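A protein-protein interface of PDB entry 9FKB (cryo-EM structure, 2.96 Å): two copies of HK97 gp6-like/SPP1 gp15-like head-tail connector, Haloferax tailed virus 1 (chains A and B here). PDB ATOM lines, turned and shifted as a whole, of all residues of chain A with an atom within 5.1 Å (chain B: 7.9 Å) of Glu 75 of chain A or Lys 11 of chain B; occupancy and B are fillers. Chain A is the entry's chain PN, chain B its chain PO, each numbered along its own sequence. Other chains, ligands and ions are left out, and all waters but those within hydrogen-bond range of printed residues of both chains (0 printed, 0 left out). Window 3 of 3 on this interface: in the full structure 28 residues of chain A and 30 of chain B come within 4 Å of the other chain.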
ATOM      1  N   SER A   5     -11.674  -6.031 -20.373  1.00  0.00           N
ATOM      2  CA  SER A   5     -10.540  -6.916 -20.625  1.00  0.00           C
ATOM      3  C   SER A   5      -9.711  -7.144 -19.350  1.00  0.00           C
ATOM      4  O   SER A   5      -9.661  -6.291 -18.469  1.00  0.00           O
ATOM      5  CB  SER A   5      -9.715  -6.391 -21.782  1.00  0.00           C
ATOM      6  OG  SER A   5      -8.623  -7.238 -22.063  1.00  0.00           O
ATOM      7  N   ILE A   6      -9.011  -8.283 -19.264  1.00  0.00           N
ATOM      8  CA  ILE A   6      -8.226  -8.693 -18.098  1.00  0.00           C
ATOM      9  C   ILE A   6      -7.118  -7.687 -17.719  1.00  0.00           C
ATOM     10  O   ILE A   6      -6.681  -7.628 -16.566  1.00  0.00           O
ATOM     11  CB  ILE A   6      -7.670 -10.111 -18.354  1.00  0.00           C
ATOM     12  CG1 ILE A   6      -7.215 -10.796 -17.061  1.00  0.00           C
ATOM     13  CG2 ILE A   6      -6.569 -10.093 -19.408  1.00  0.00           C
ATOM     14  CD1 ILE A   6      -6.801 -12.246 -17.218  1.00  0.00           C
ATOM     15  N   ASP A   7      -6.641  -6.895 -18.689  1.00  0.00           N
ATOM     16  CA  ASP A   7      -5.638  -5.851 -18.502  1.00  0.00           C
ATOM     17  C   ASP A   7      -6.245  -4.495 -18.108  1.00  0.00           C
ATOM     18  O   ASP A   7      -5.520  -3.593 -17.684  1.00  0.00           O
ATOM     19  CB  ASP A   7      -4.748  -5.723 -19.742  1.00  0.00           C
ATOM     20  CG  ASP A   7      -5.469  -5.447 -21.061  1.00  0.00           C
ATOM     21  OD1 ASP A   7      -6.630  -5.864 -21.210  1.00  0.00           O
ATOM     22  OD2 ASP A   7      -4.844  -4.824 -21.954  1.00  0.00           O
ATOM     23  N   GLN A  28     -12.051 -17.174 -21.079  1.00  0.00           N
ATOM     24  CA  GLN A  28     -10.907 -16.857 -21.918  1.00  0.00           C
ATOM     25  C   GLN A  28      -9.646 -17.593 -21.447  1.00  0.00           C
ATOM     26  O   GLN A  28      -8.984 -18.229 -22.264  1.00  0.00           O
ATOM     27  CB  GLN A  28     -10.699 -15.349 -22.008  1.00  0.00           C
ATOM     28  CG  GLN A  28      -9.640 -14.985 -23.042  1.00  0.00           C
ATOM     29  CD  GLN A  28      -9.442 -13.505 -23.270  1.00  0.00           C
ATOM     30  OE1 GLN A  28      -9.932 -12.660 -22.521  1.00  0.00           O
ATOM     31  NE2 GLN A  28      -8.722 -13.166 -24.331  1.00  0.00           N
ATOM     32  N   ASP A  73       1.821  -7.557 -24.779  1.00  0.00           N
ATOM     33  CA  ASP A  73       0.400  -7.316 -24.528  1.00  0.00           C
ATOM     34  C   ASP A  73      -0.009  -7.755 -23.114  1.00  0.00           C
ATOM     35  O   ASP A  73      -0.005  -8.946 -22.806  1.00  0.00           O
ATOM     36  CB  ASP A  73      -0.462  -7.969 -25.615  1.00  0.00           C
ATOM     37  CG  ASP A  73      -1.950  -7.676 -25.495  1.00  0.00           C
ATOM     38  OD1 ASP A  73      -2.356  -7.009 -24.521  1.00  0.00           O
ATOM     39  OD2 ASP A  73      -2.696  -8.108 -26.387  1.00  0.00           O
ATOM     40  N   ALA A  74      -0.442  -6.796 -22.279  1.00  0.00           N
ATOM     41  CA  ALA A  74      -0.824  -7.047 -20.894  1.00  0.00           C
ATOM     42  C   ALA A  74      -2.040  -7.969 -20.751  1.00  0.00           C
ATOM     43  O   ALA A  74      -2.193  -8.610 -19.709  1.00  0.00           O
ATOM     44  CB  ALA A  74      -1.039  -5.740 -20.175  1.00  0.00           C
ATOM     45  N   GLU A  75      -2.889  -8.073 -21.784  1.00  0.00           N
ATOM     46  CA  GLU A  75      -3.952  -9.074 -21.814  1.00  0.00           C
ATOM     47  C   GLU A  75      -3.325 -10.466 -21.735  1.00  0.00           C
ATOM     48  O   GLU A  75      -3.465 -11.172 -20.736  1.00  0.00           O
ATOM     49  CB  GLU A  75      -4.825  -8.883 -23.059  1.00  0.00           C
ATOM     50  CG  GLU A  75      -5.907  -9.937 -23.256  1.00  0.00           C
ATOM     51  CD  GLU A  75      -6.806  -9.722 -24.467  1.00  0.00           C
ATOM     52  OE1 GLU A  75      -6.560  -8.767 -25.231  1.00  0.00           O
ATOM     53  OE2 GLU A  75      -7.796 -10.480 -24.611  1.00  0.00           O
ATOM     54  N   TYR A  76      -2.555 -10.819 -22.771  1.00  0.00           N
ATOM     55  CA  TYR A  76      -1.924 -12.123 -22.868  1.00  0.00           C
ATOM     56  C   TYR A  76      -0.916 -12.385 -21.757  1.00  0.00           C
ATOM     57  O   TYR A  76      -0.850 -13.512 -21.290  1.00  0.00           O
ATOM     58  CB  TYR A  76      -1.370 -12.362 -24.266  1.00  0.00           C
ATOM     59  CG  TYR A  76      -2.474 -12.757 -25.204  1.00  0.00           C
ATOM     60  CD1 TYR A  76      -3.060 -14.010 -25.119  1.00  0.00           C
ATOM     61  CD2 TYR A  76      -2.996 -11.861 -26.125  1.00  0.00           C
ATOM     62  CE1 TYR A  76      -4.147 -14.359 -25.911  1.00  0.00           C
ATOM     63  CE2 TYR A  76      -4.045 -12.215 -26.973  1.00  0.00           C
ATOM     64  CZ  TYR A  76      -4.618 -13.476 -26.876  1.00  0.00           C
ATOM     65  OH  TYR A  76      -5.650 -13.820 -27.712  1.00  0.00           O
ATOM     66  N   PHE A  77      -0.179 -11.376 -21.282  1.00  0.00           N
ATOM     67  CA  PHE A  77       0.653 -11.576 -20.103  1.00  0.00           C
ATOM     68  C   PHE A  77      -0.175 -12.054 -18.904  1.00  0.00           C
ATOM     69  O   PHE A  77       0.187 -13.030 -18.248  1.00  0.00           O
ATOM     70  CB  PHE A  77       1.449 -10.323 -19.743  1.00  0.00           C
ATOM     71  CG  PHE A  77       2.233 -10.486 -18.460  1.00  0.00           C
ATOM     72  CD1 PHE A  77       3.305 -11.367 -18.390  1.00  0.00           C
ATOM     73  CD2 PHE A  77       1.884  -9.801 -17.299  1.00  0.00           C
ATOM     74  CE1 PHE A  77       4.009 -11.561 -17.208  1.00  0.00           C
ATOM     75  CE2 PHE A  77       2.608  -9.970 -16.119  1.00  0.00           C
ATOM     76  CZ  PHE A  77       3.674 -10.844 -16.079  1.00  0.00           C
ATOM     77  N   THR A  78      -1.312 -11.408 -18.627  1.00  0.00           N
ATOM     78  CA  THR A  78      -2.145 -11.826 -17.507  1.00  0.00           C
ATOM     79  C   THR A  78      -2.773 -13.203 -17.753  1.00  0.00           C
ATOM     80  O   THR A  78      -2.891 -14.003 -16.831  1.00  0.00           O
ATOM     81  CB  THR A  78      -3.235 -10.809 -17.148  1.00  0.00           C
ATOM     82  OG1 THR A  78      -2.727  -9.477 -17.206  1.00  0.00           O
ATOM     83  CG2 THR A  78      -3.732 -11.005 -15.731  1.00  0.00           C
ATOM     84  N   LEU A  79      -3.158 -13.512 -18.995  1.00  0.00           N
ATOM     85  CA  LEU A  79      -3.662 -14.836 -19.349  1.00  0.00           C
ATOM     86  C   LEU A  79      -2.603 -15.908 -19.085  1.00  0.00           C
ATOM     87  O   LEU A  79      -2.884 -16.858 -18.356  1.00  0.00           O
ATOM     88  CB  LEU A  79      -4.161 -14.875 -20.798  1.00  0.00           C
ATOM     89  CG  LEU A  79      -5.347 -13.966 -21.130  1.00  0.00           C
ATOM     90  CD1 LEU A  79      -5.643 -13.988 -22.629  1.00  0.00           C
ATOM     91  CD2 LEU A  79      -6.600 -14.381 -20.364  1.00  0.00           C
ATOM     92  N   VAL B   9      -3.244  -8.502 -40.725  1.00  0.00           N
ATOM     93  CA  VAL B   9      -4.158  -8.278 -39.604  1.00  0.00           C
ATOM     94  C   VAL B   9      -3.397  -8.077 -38.286  1.00  0.00           C
ATOM     95  O   VAL B   9      -2.343  -8.679 -38.051  1.00  0.00           O
ATOM     96  CB  VAL B   9      -5.207  -9.407 -39.499  1.00  0.00           C
ATOM     97  CG1 VAL B   9      -6.222  -9.328 -40.631  1.00  0.00           C
ATOM     98  CG2 VAL B   9      -4.578 -10.798 -39.429  1.00  0.00           C
ATOM     99  N   SER B  10      -3.967  -7.229 -37.407  1.00  0.00           N
ATOM    100  CA  SER B  10      -3.590  -7.045 -36.005  1.00  0.00           C
ATOM    101  C   SER B  10      -4.710  -7.553 -35.077  1.00  0.00           C
ATOM    102  O   SER B  10      -5.742  -8.023 -35.551  1.00  0.00           O
ATOM    103  CB  SER B  10      -3.249  -5.593 -35.759  1.00  0.00           C
ATOM    104  OG  SER B  10      -2.624  -5.419 -34.496  1.00  0.00           O
ATOM    105  N   LYS B  11      -4.544  -7.449 -33.744  1.00  0.00           N
ATOM    106  CA  LYS B  11      -5.489  -8.008 -32.776  1.00  0.00           C
ATOM    107  C   LYS B  11      -6.909  -7.453 -32.952  1.00  0.00           C
ATOM    108  O   LYS B  11      -7.886  -8.214 -32.994  1.00  0.00           O
ATOM    109  CB  LYS B  11      -4.958  -7.858 -31.349  1.00  0.00           C
ATOM    110  CG  LYS B  11      -5.840  -8.520 -30.298  1.00  0.00           C
ATOM    111  CD  LYS B  11      -5.345  -8.377 -28.867  1.00  0.00           C
ATOM    112  CE  LYS B  11      -5.381  -6.940 -28.370  1.00  0.00           C
ATOM    113  NZ  LYS B  11      -4.951  -6.796 -26.955  1.00  0.00           N
ATOM    114  N   SER B  12      -7.021  -6.125 -33.083  1.00  0.00           N
ATOM    115  CA  SER B  12      -8.286  -5.439 -33.319  1.00  0.00           C
ATOM    116  C   SER B  12      -8.945  -5.831 -34.652  1.00  0.00           C
ATOM    117  O   SER B  12     -10.176  -5.791 -34.762  1.00  0.00           O
ATOM    118  CB  SER B  12      -8.105  -3.950 -33.206  1.00  0.00           C
ATOM    119  OG  SER B  12      -7.154  -3.502 -34.158  1.00  0.00           O
ATOM    120  N   ASP B  13      -8.145  -6.231 -35.655  1.00  0.00           N
ATOM    121  CA  ASP B  13      -8.647  -6.740 -36.927  1.00  0.00           C
ATOM    122  C   ASP B  13      -9.169  -8.168 -36.781  1.00  0.00           C
ATOM    123  O   ASP B  13     -10.262  -8.468 -37.260  1.00  0.00           O
ATOM    124  CB  ASP B  13      -7.582  -6.697 -38.022  1.00  0.00           C
ATOM    125  CG  ASP B  13      -6.980  -5.322 -38.236  1.00  0.00           C
ATOM    126  OD1 ASP B  13      -7.762  -4.355 -38.341  1.00  0.00           O
ATOM    127  OD2 ASP B  13      -5.729  -5.228 -38.303  1.00  0.00           O
ATOM    128  N   TRP B  14      -8.402  -9.032 -36.104  1.00  0.00           N
ATOM    129  CA  TRP B  14      -8.772 -10.424 -35.873  1.00  0.00           C
ATOM    130  C   TRP B  14     -10.149 -10.544 -35.212  1.00  0.00           C
ATOM    131  O   TRP B  14     -10.968 -11.358 -35.639  1.00  0.00           O
ATOM    132  CB  TRP B  14      -7.679 -11.109 -35.054  1.00  0.00           C
ATOM    133  CG  TRP B  14      -7.994 -12.534 -34.708  1.00  0.00           C
ATOM    134  CD1 TRP B  14      -8.652 -12.957 -33.594  1.00  0.00           C
ATOM    135  CD2 TRP B  14      -7.729 -13.725 -35.493  1.00  0.00           C
ATOM    136  NE1 TRP B  14      -8.788 -14.321 -33.618  1.00  0.00           N
ATOM    137  CE2 TRP B  14      -8.220 -14.835 -34.764  1.00  0.00           C
ATOM    138  CE3 TRP B  14      -7.143 -13.976 -36.747  1.00  0.00           C
ATOM    139  CZ2 TRP B  14      -8.102 -16.158 -35.237  1.00  0.00           C
ATOM    140  CZ3 TRP B  14      -7.052 -15.275 -37.232  1.00  0.00           C
ATOM    141  CH2 TRP B  14      -7.523 -16.354 -36.477  1.00  0.00           C
ATOM    142  N   ASP B  15     -10.410  -9.720 -34.191  1.00  0.00           N
ATOM    143  CA  ASP B  15     -11.697  -9.633 -33.508  1.00  0.00           C
ATOM    144  C   ASP B  15     -12.848  -9.114 -34.390  1.00  0.00           C
ATOM    145  O   ASP B  15     -14.011  -9.189 -33.979  1.00  0.00           O
ATOM    146  CB  ASP B  15     -11.553  -8.808 -32.226  1.00  0.00           C
ATOM    147  CG  ASP B  15     -10.771  -9.489 -31.109  1.00  0.00           C
ATOM    148  OD1 ASP B  15     -10.468 -10.699 -31.232  1.00  0.00           O
ATOM    149  OD2 ASP B  15     -10.482  -8.815 -30.092  1.00  0.00           O
ATOM    150  N   ALA B  16     -12.536  -8.597 -35.592  1.00  0.00           N
ATOM    151  CA  ALA B  16     -13.504  -8.053 -36.541  1.00  0.00           C
ATOM    152  C   ALA B  16     -13.598  -8.857 -37.852  1.00  0.00           C
ATOM    153  O   ALA B  16     -14.476  -8.578 -38.671  1.00  0.00           O
ATOM    154  CB  ALA B  16     -13.190  -6.592 -36.779  1.00  0.00           C
ATOM    155  N   LEU B  17     -12.737  -9.873 -38.052  1.00  0.00           N
ATOM    156  CA  LEU B  17     -12.855 -10.794 -39.179  1.00  0.00           C
ATOM    157  C   LEU B  17     -14.157 -11.599 -39.085  1.00  0.00           C
ATOM    158  O   LEU B  17     -14.627 -11.916 -37.991  1.00  0.00           O
ATOM    159  CB  LEU B  17     -11.660 -11.754 -39.210  1.00  0.00           C
ATOM    160  CG  LEU B  17     -10.281 -11.167 -39.523  1.00  0.00           C
ATOM    161  CD1 LEU B  17      -9.233 -12.268 -39.435  1.00  0.00           C
ATOM    162  CD2 LEU B  17     -10.238 -10.529 -40.909  1.00  0.00           C
ATOM    163  N   GLN B  22     -11.444 -15.811 -40.595  1.00  0.00           N
ATOM    164  CA  GLN B  22     -10.749 -16.301 -39.418  1.00  0.00           C
ATOM    165  C   GLN B  22     -10.446 -17.802 -39.568  1.00  0.00           C
ATOM    166  O   GLN B  22      -9.335 -18.249 -39.269  1.00  0.00           O
ATOM    167  CB  GLN B  22     -11.637 -15.928 -38.234  1.00  0.00           C
ATOM    168  CG  GLN B  22     -10.922 -15.764 -36.906  1.00  0.00           C
ATOM    169  CD  GLN B  22     -11.892 -15.426 -35.794  1.00  0.00           C
ATOM    170  OE1 GLN B  22     -12.683 -16.254 -35.355  1.00  0.00           O
ATOM    171  NE2 GLN B  22     -11.852 -14.202 -35.302  1.00  0.00           N
ATOM    172  N   GLU B  47      -7.674 -18.463 -30.154  1.00  0.00           N
ATOM    173  CA  GLU B  47      -6.948 -17.798 -29.074  1.00  0.00           C
ATOM    174  C   GLU B  47      -5.432 -17.842 -29.289  1.00  0.00           C
ATOM    175  O   GLU B  47      -4.749 -16.834 -29.107  1.00  0.00           O
ATOM    176  CB  GLU B  47      -7.302 -18.434 -27.727  1.00  0.00           C
ATOM    177  CG  GLU B  47      -7.012 -17.521 -26.551  1.00  0.00           C
ATOM    178  CD  GLU B  47      -8.143 -16.533 -26.271  1.00  0.00           C
ATOM    179  OE1 GLU B  47      -9.311 -16.970 -26.121  1.00  0.00           O
ATOM    180  OE2 GLU B  47      -7.859 -15.314 -26.213  1.00  0.00           O
ATOM    181  N   ILE B  49      -3.798 -18.114 -32.222  1.00  0.00           N
ATOM    182  CA  ILE B  49      -3.477 -17.253 -33.359  1.00  0.00           C
ATOM    183  C   ILE B  49      -3.572 -15.778 -32.961  1.00  0.00           C
ATOM    184  O   ILE B  49      -2.654 -15.007 -33.219  1.00  0.00           O
ATOM    185  CB  ILE B  49      -4.356 -17.578 -34.582  1.00  0.00           C
ATOM    186  CG1 ILE B  49      -3.992 -18.947 -35.160  1.00  0.00           C
ATOM    187  CG2 ILE B  49      -4.217 -16.509 -35.660  1.00  0.00           C
ATOM    188  CD1 ILE B  49      -5.111 -19.584 -35.973  1.00  0.00           C
ATOM    189  N   ARG B  50      -4.661 -15.380 -32.296  1.00  0.00           N
ATOM    190  CA  ARG B  50      -4.844 -14.026 -31.784  1.00  0.00           C
ATOM    191  C   ARG B  50      -3.690 -13.620 -30.861  1.00  0.00           C
ATOM    192  O   ARG B  50      -3.169 -12.515 -30.968  1.00  0.00           O
ATOM    193  CB  ARG B  50      -6.181 -13.970 -31.044  1.00  0.00           C
ATOM    194  CG  ARG B  50      -6.577 -12.574 -30.605  1.00  0.00           C
ATOM    195  CD  ARG B  50      -7.905 -12.665 -29.909  1.00  0.00           C
ATOM    196  NE  ARG B  50      -8.499 -11.428 -29.431  1.00  0.00           N
ATOM    197  CZ  ARG B  50      -8.348 -10.885 -28.228  1.00  0.00           C
ATOM    198  NH1 ARG B  50      -9.036  -9.798 -27.915  1.00  0.00           N
ATOM    199  NH2 ARG B  50      -7.517 -11.420 -27.347  1.00  0.00           N
ATOM    200  N   SER B  51      -3.257 -14.537 -29.989  1.00  0.00           N
ATOM    201  CA  SER B  51      -2.095 -14.353 -29.132  1.00  0.00           C
ATOM    202  C   SER B  51      -0.805 -14.204 -29.938  1.00  0.00           C
ATOM    203  O   SER B  51      -0.011 -13.322 -29.644  1.00  0.00           O
ATOM    204  CB  SER B  51      -1.971 -15.462 -28.123  1.00  0.00           C
ATOM    205  OG  SER B  51      -1.001 -15.135 -27.138  1.00  0.00           O
ATOM    206  N   ILE B  53      -0.540 -13.073 -33.070  1.00  0.00           N
ATOM    207  CA  ILE B  53      -0.677 -11.762 -33.694  1.00  0.00           C
ATOM    208  C   ILE B  53      -0.322 -10.648 -32.705  1.00  0.00           C
ATOM    209  O   ILE B  53       0.541  -9.824 -32.987  1.00  0.00           O
ATOM    210  CB  ILE B  53      -2.092 -11.630 -34.292  1.00  0.00           C
ATOM    211  CG1 ILE B  53      -2.210 -12.481 -35.559  1.00  0.00           C
ATOM    212  CG2 ILE B  53      -2.483 -10.174 -34.550  1.00  0.00           C
ATOM    213  CD1 ILE B  53      -3.632 -12.721 -36.037  1.00  0.00           C
ATOM    214  N   ALA B  54      -0.944 -10.646 -31.524  1.00  0.00           N
ATOM    215  CA  ALA B  54      -0.701  -9.653 -30.482  1.00  0.00           C
ATOM    216  C   ALA B  54       0.753  -9.675 -29.984  1.00  0.00           C
ATOM    217  O   ALA B  54       1.359  -8.635 -29.739  1.00  0.00           O
ATOM    218  CB  ALA B  54      -1.681  -9.905 -29.367  1.00  0.00           C
ATOM    219  N   GLU B  55       1.329 -10.870 -29.849  1.00  0.00           N
ATOM    220  CA  GLU B  55       2.705 -11.058 -29.423  1.00  0.00           C
ATOM    221  C   GLU B  55       3.679 -10.536 -30.479  1.00  0.00           C
ATOM    222  O   GLU B  55       4.599  -9.801 -30.134  1.00  0.00           O
ATOM    223  CB  GLU B  55       2.938 -12.529 -29.097  1.00  0.00           C
ATOM    224  CG  GLU B  55       4.306 -12.809 -28.499  1.00  0.00           C
ATOM    225  CD  GLU B  55       4.366 -14.162 -27.804  1.00  0.00           C
ATOM    226  OE1 GLU B  55       3.596 -14.376 -26.844  1.00  0.00           O
ATOM    227  OE2 GLU B  55       5.151 -15.031 -28.242  1.00  0.00           O
ATOM    228  N   ARG B  56       3.454 -10.842 -31.760  1.00  0.00           N
ATOM    229  CA  ARG B  56       4.242 -10.295 -32.861  1.00  0.00           C
ATOM    230  C   ARG B  56       4.227  -8.766 -32.824  1.00  0.00           C
ATOM    231  O   ARG B  56       5.275  -8.134 -32.777  1.00  0.00           O
ATOM    232  CB  ARG B  56       3.711 -10.805 -34.205  1.00  0.00           C
ATOM    233  CG  ARG B  56       4.429 -10.240 -35.424  1.00  0.00           C
ATOM    234  CD  ARG B  56       3.617 -10.451 -36.690  1.00  0.00           C
ATOM    235  NE  ARG B  56       2.433  -9.610 -36.696  1.00  0.00           N
ATOM    236  CZ  ARG B  56       1.257  -9.856 -37.279  1.00  0.00           C
ATOM    237  NH1 ARG B  56       0.301  -8.956 -37.162  1.00  0.00           N
ATOM    238  NH2 ARG B  56       1.014 -10.963 -37.959  1.00  0.00           N
ATOM    239  N   ASP B  57       3.035  -8.176 -32.816  1.00  0.00           N
ATOM    240  CA  ASP B  57       2.885  -6.734 -32.904  1.00  0.00           C
ATOM    241  C   ASP B  57       3.468  -5.996 -31.688  1.00  0.00           C
ATOM    242  O   ASP B  57       3.760  -4.805 -31.805  1.00  0.00           O
ATOM    243  CB  ASP B  57       1.421  -6.367 -33.159  1.00  0.00           C
ATOM    244  CG  ASP B  57       0.880  -6.757 -34.529  1.00  0.00           C
ATOM    245  OD1 ASP B  57       1.671  -7.246 -35.374  1.00  0.00           O
ATOM    246  OD2 ASP B  57      -0.338  -6.545 -34.757  1.00  0.00           O
ATOM    247  N   THR B  58       3.664  -6.672 -30.540  1.00  0.00           N
ATOM    248  CA  THR B  58       4.208  -6.054 -29.327  1.00  0.00           C
ATOM    249  C   THR B  58       5.661  -6.454 -29.043  1.00  0.00           C
ATOM    250  O   THR B  58       6.518  -5.577 -28.970  1.00  0.00           O
ATOM    251  CB  THR B  58       3.301  -6.255 -28.104  1.00  0.00           C
ATOM    252  OG1 THR B  58       3.076  -7.649 -27.891  1.00  0.00           O
ATOM    253  CG2 THR B  58       1.969  -5.549 -28.228  1.00  0.00           C
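The guanidinium group (NH2) of Arg 50 of chain B sits at hydrogen-bond distance from the side-chain hydroxyl (OH) of Tyr 76 of chain A.
The side-chain amino group of Lys 11 of chain B lies within salt-bridge range of the side-chain carboxylate of Asp 73 of chain A, at 2.7 Å.
OE2 of Glu 75 of chain A is in salt-bridge range of NH2 of Arg 50 of chain B, 2.9 Å away.
OH of Tyr 76 of chain A lies within hydrogen-bond range of OE2 of Glu 47 of chain B (3.1 Å).
The backbone NH (N) of Asp 73 of chain A sits at hydrogen-bond distance from the side-chain hydroxyl (OG1) of Thr 58 of chain B, at 3.4 Å.
The backbone NH (N) of Ser 51 of chain B sits at hydrogen-bond distance from the side-chain hydroxyl (OH) of Tyr 76 of chain A (3.4 Å).
The side-chain carboxylate of Glu 75 of chain A lies within salt-bridge range of the side-chain amino group of Lys 11 of chain B, 3.1 Å away.
NE2 of Gln 28 of chain A is in hydrogen-bond range of OE2 of Glu 47 of chain B, at 3.0 Å.
The backbone carbonyl oxygen of Ala 54 of chain B lies within hydrogen-bond range of the side-chain hydroxyl of Thr 58 of chain B, at 2.7 Å.
N of Glu 75 of chain A lies within hydrogen-bond range of OD1 of Asp 73 of chain A, 3.0 Å away.
The side-chain carboxylate of Asp 15 of chain B is in salt-bridge range of the guanidinium group of Arg 50 of chain B (2.8 Å).
NE2 of Gln 28 of chain A lies within hydrogen-bond range of OE2 of Glu 75 of chain A (2.9 Å).
The backbone carbonyl oxygen of Glu 55 of chain B is in hydrogen-bond range of the side-chain hydroxyl of Thr 58 of chain B.
NE2 of Gln 28 of chain A touches NH2 of Arg 50 of chain B, at 3.7 Å.
OD2 of Asp 73 of chain A touches CB of Ala 54 of chain B (3.6 Å).
Glu 75 of chain A touches two residues of chain B.
Of chain A, only Asp 73 (2.7 Å) and Glu 75 (3.1 Å) come within 4 Å of Lys 11 of chain B.
No residue of chain B comes within 4 Å of Ala 74 of chain A.
Of the printed residues of chain A, Arg 50 of chain B touches Gln 28 (3.7 Å), Glu 75 (2.9 Å) and Tyr 76 (3.1 Å).
Of the printed residues of chain B, Tyr 76 of chain A touches Glu 47, Arg 50 and Ser 51.
Of the printed residues of chain B, Gln 28 of chain A touches Glu 47 (3.0 Å) and Arg 50 (3.7 Å).
Printed residues of chain A within 4 Å of Glu 47 of chain B: Gln 28 (3.0 Å) and Tyr 76 (3.1 Å).
Ser 12 of chain B touches none of the printed residues of chain A.
The nearest residue of chain B that does not touch Glu 75 of chain A is Glu 47 of chain B (5.1 Å).
The nearest printed residue of chain A that does not touch Arg 50 of chain B is Leu 79 of chain A (5.7 Å).
Hydrophobic or aromatic side chains of chain B within 4 Å of the printed part of chain A: Ala 54.
Hydrophobic or aromatic side chains of chain A within 4 Å of the printed part of chain B: Tyr 76.
Along chain A the printed residues that touch a printed residue of chain B span positions 28 to 76.
Among the printed residues, Asp or Glu carboxylates within 4 Å of a Lys or Arg side-chain nitrogen of the other chain: Asp 73 of chain A with Lys 11 of chain B, Glu 75 of chain A with Lys 11 of chain B and Glu 75 of chain A with Arg 50 of chain B.
No position is printed for both chains.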
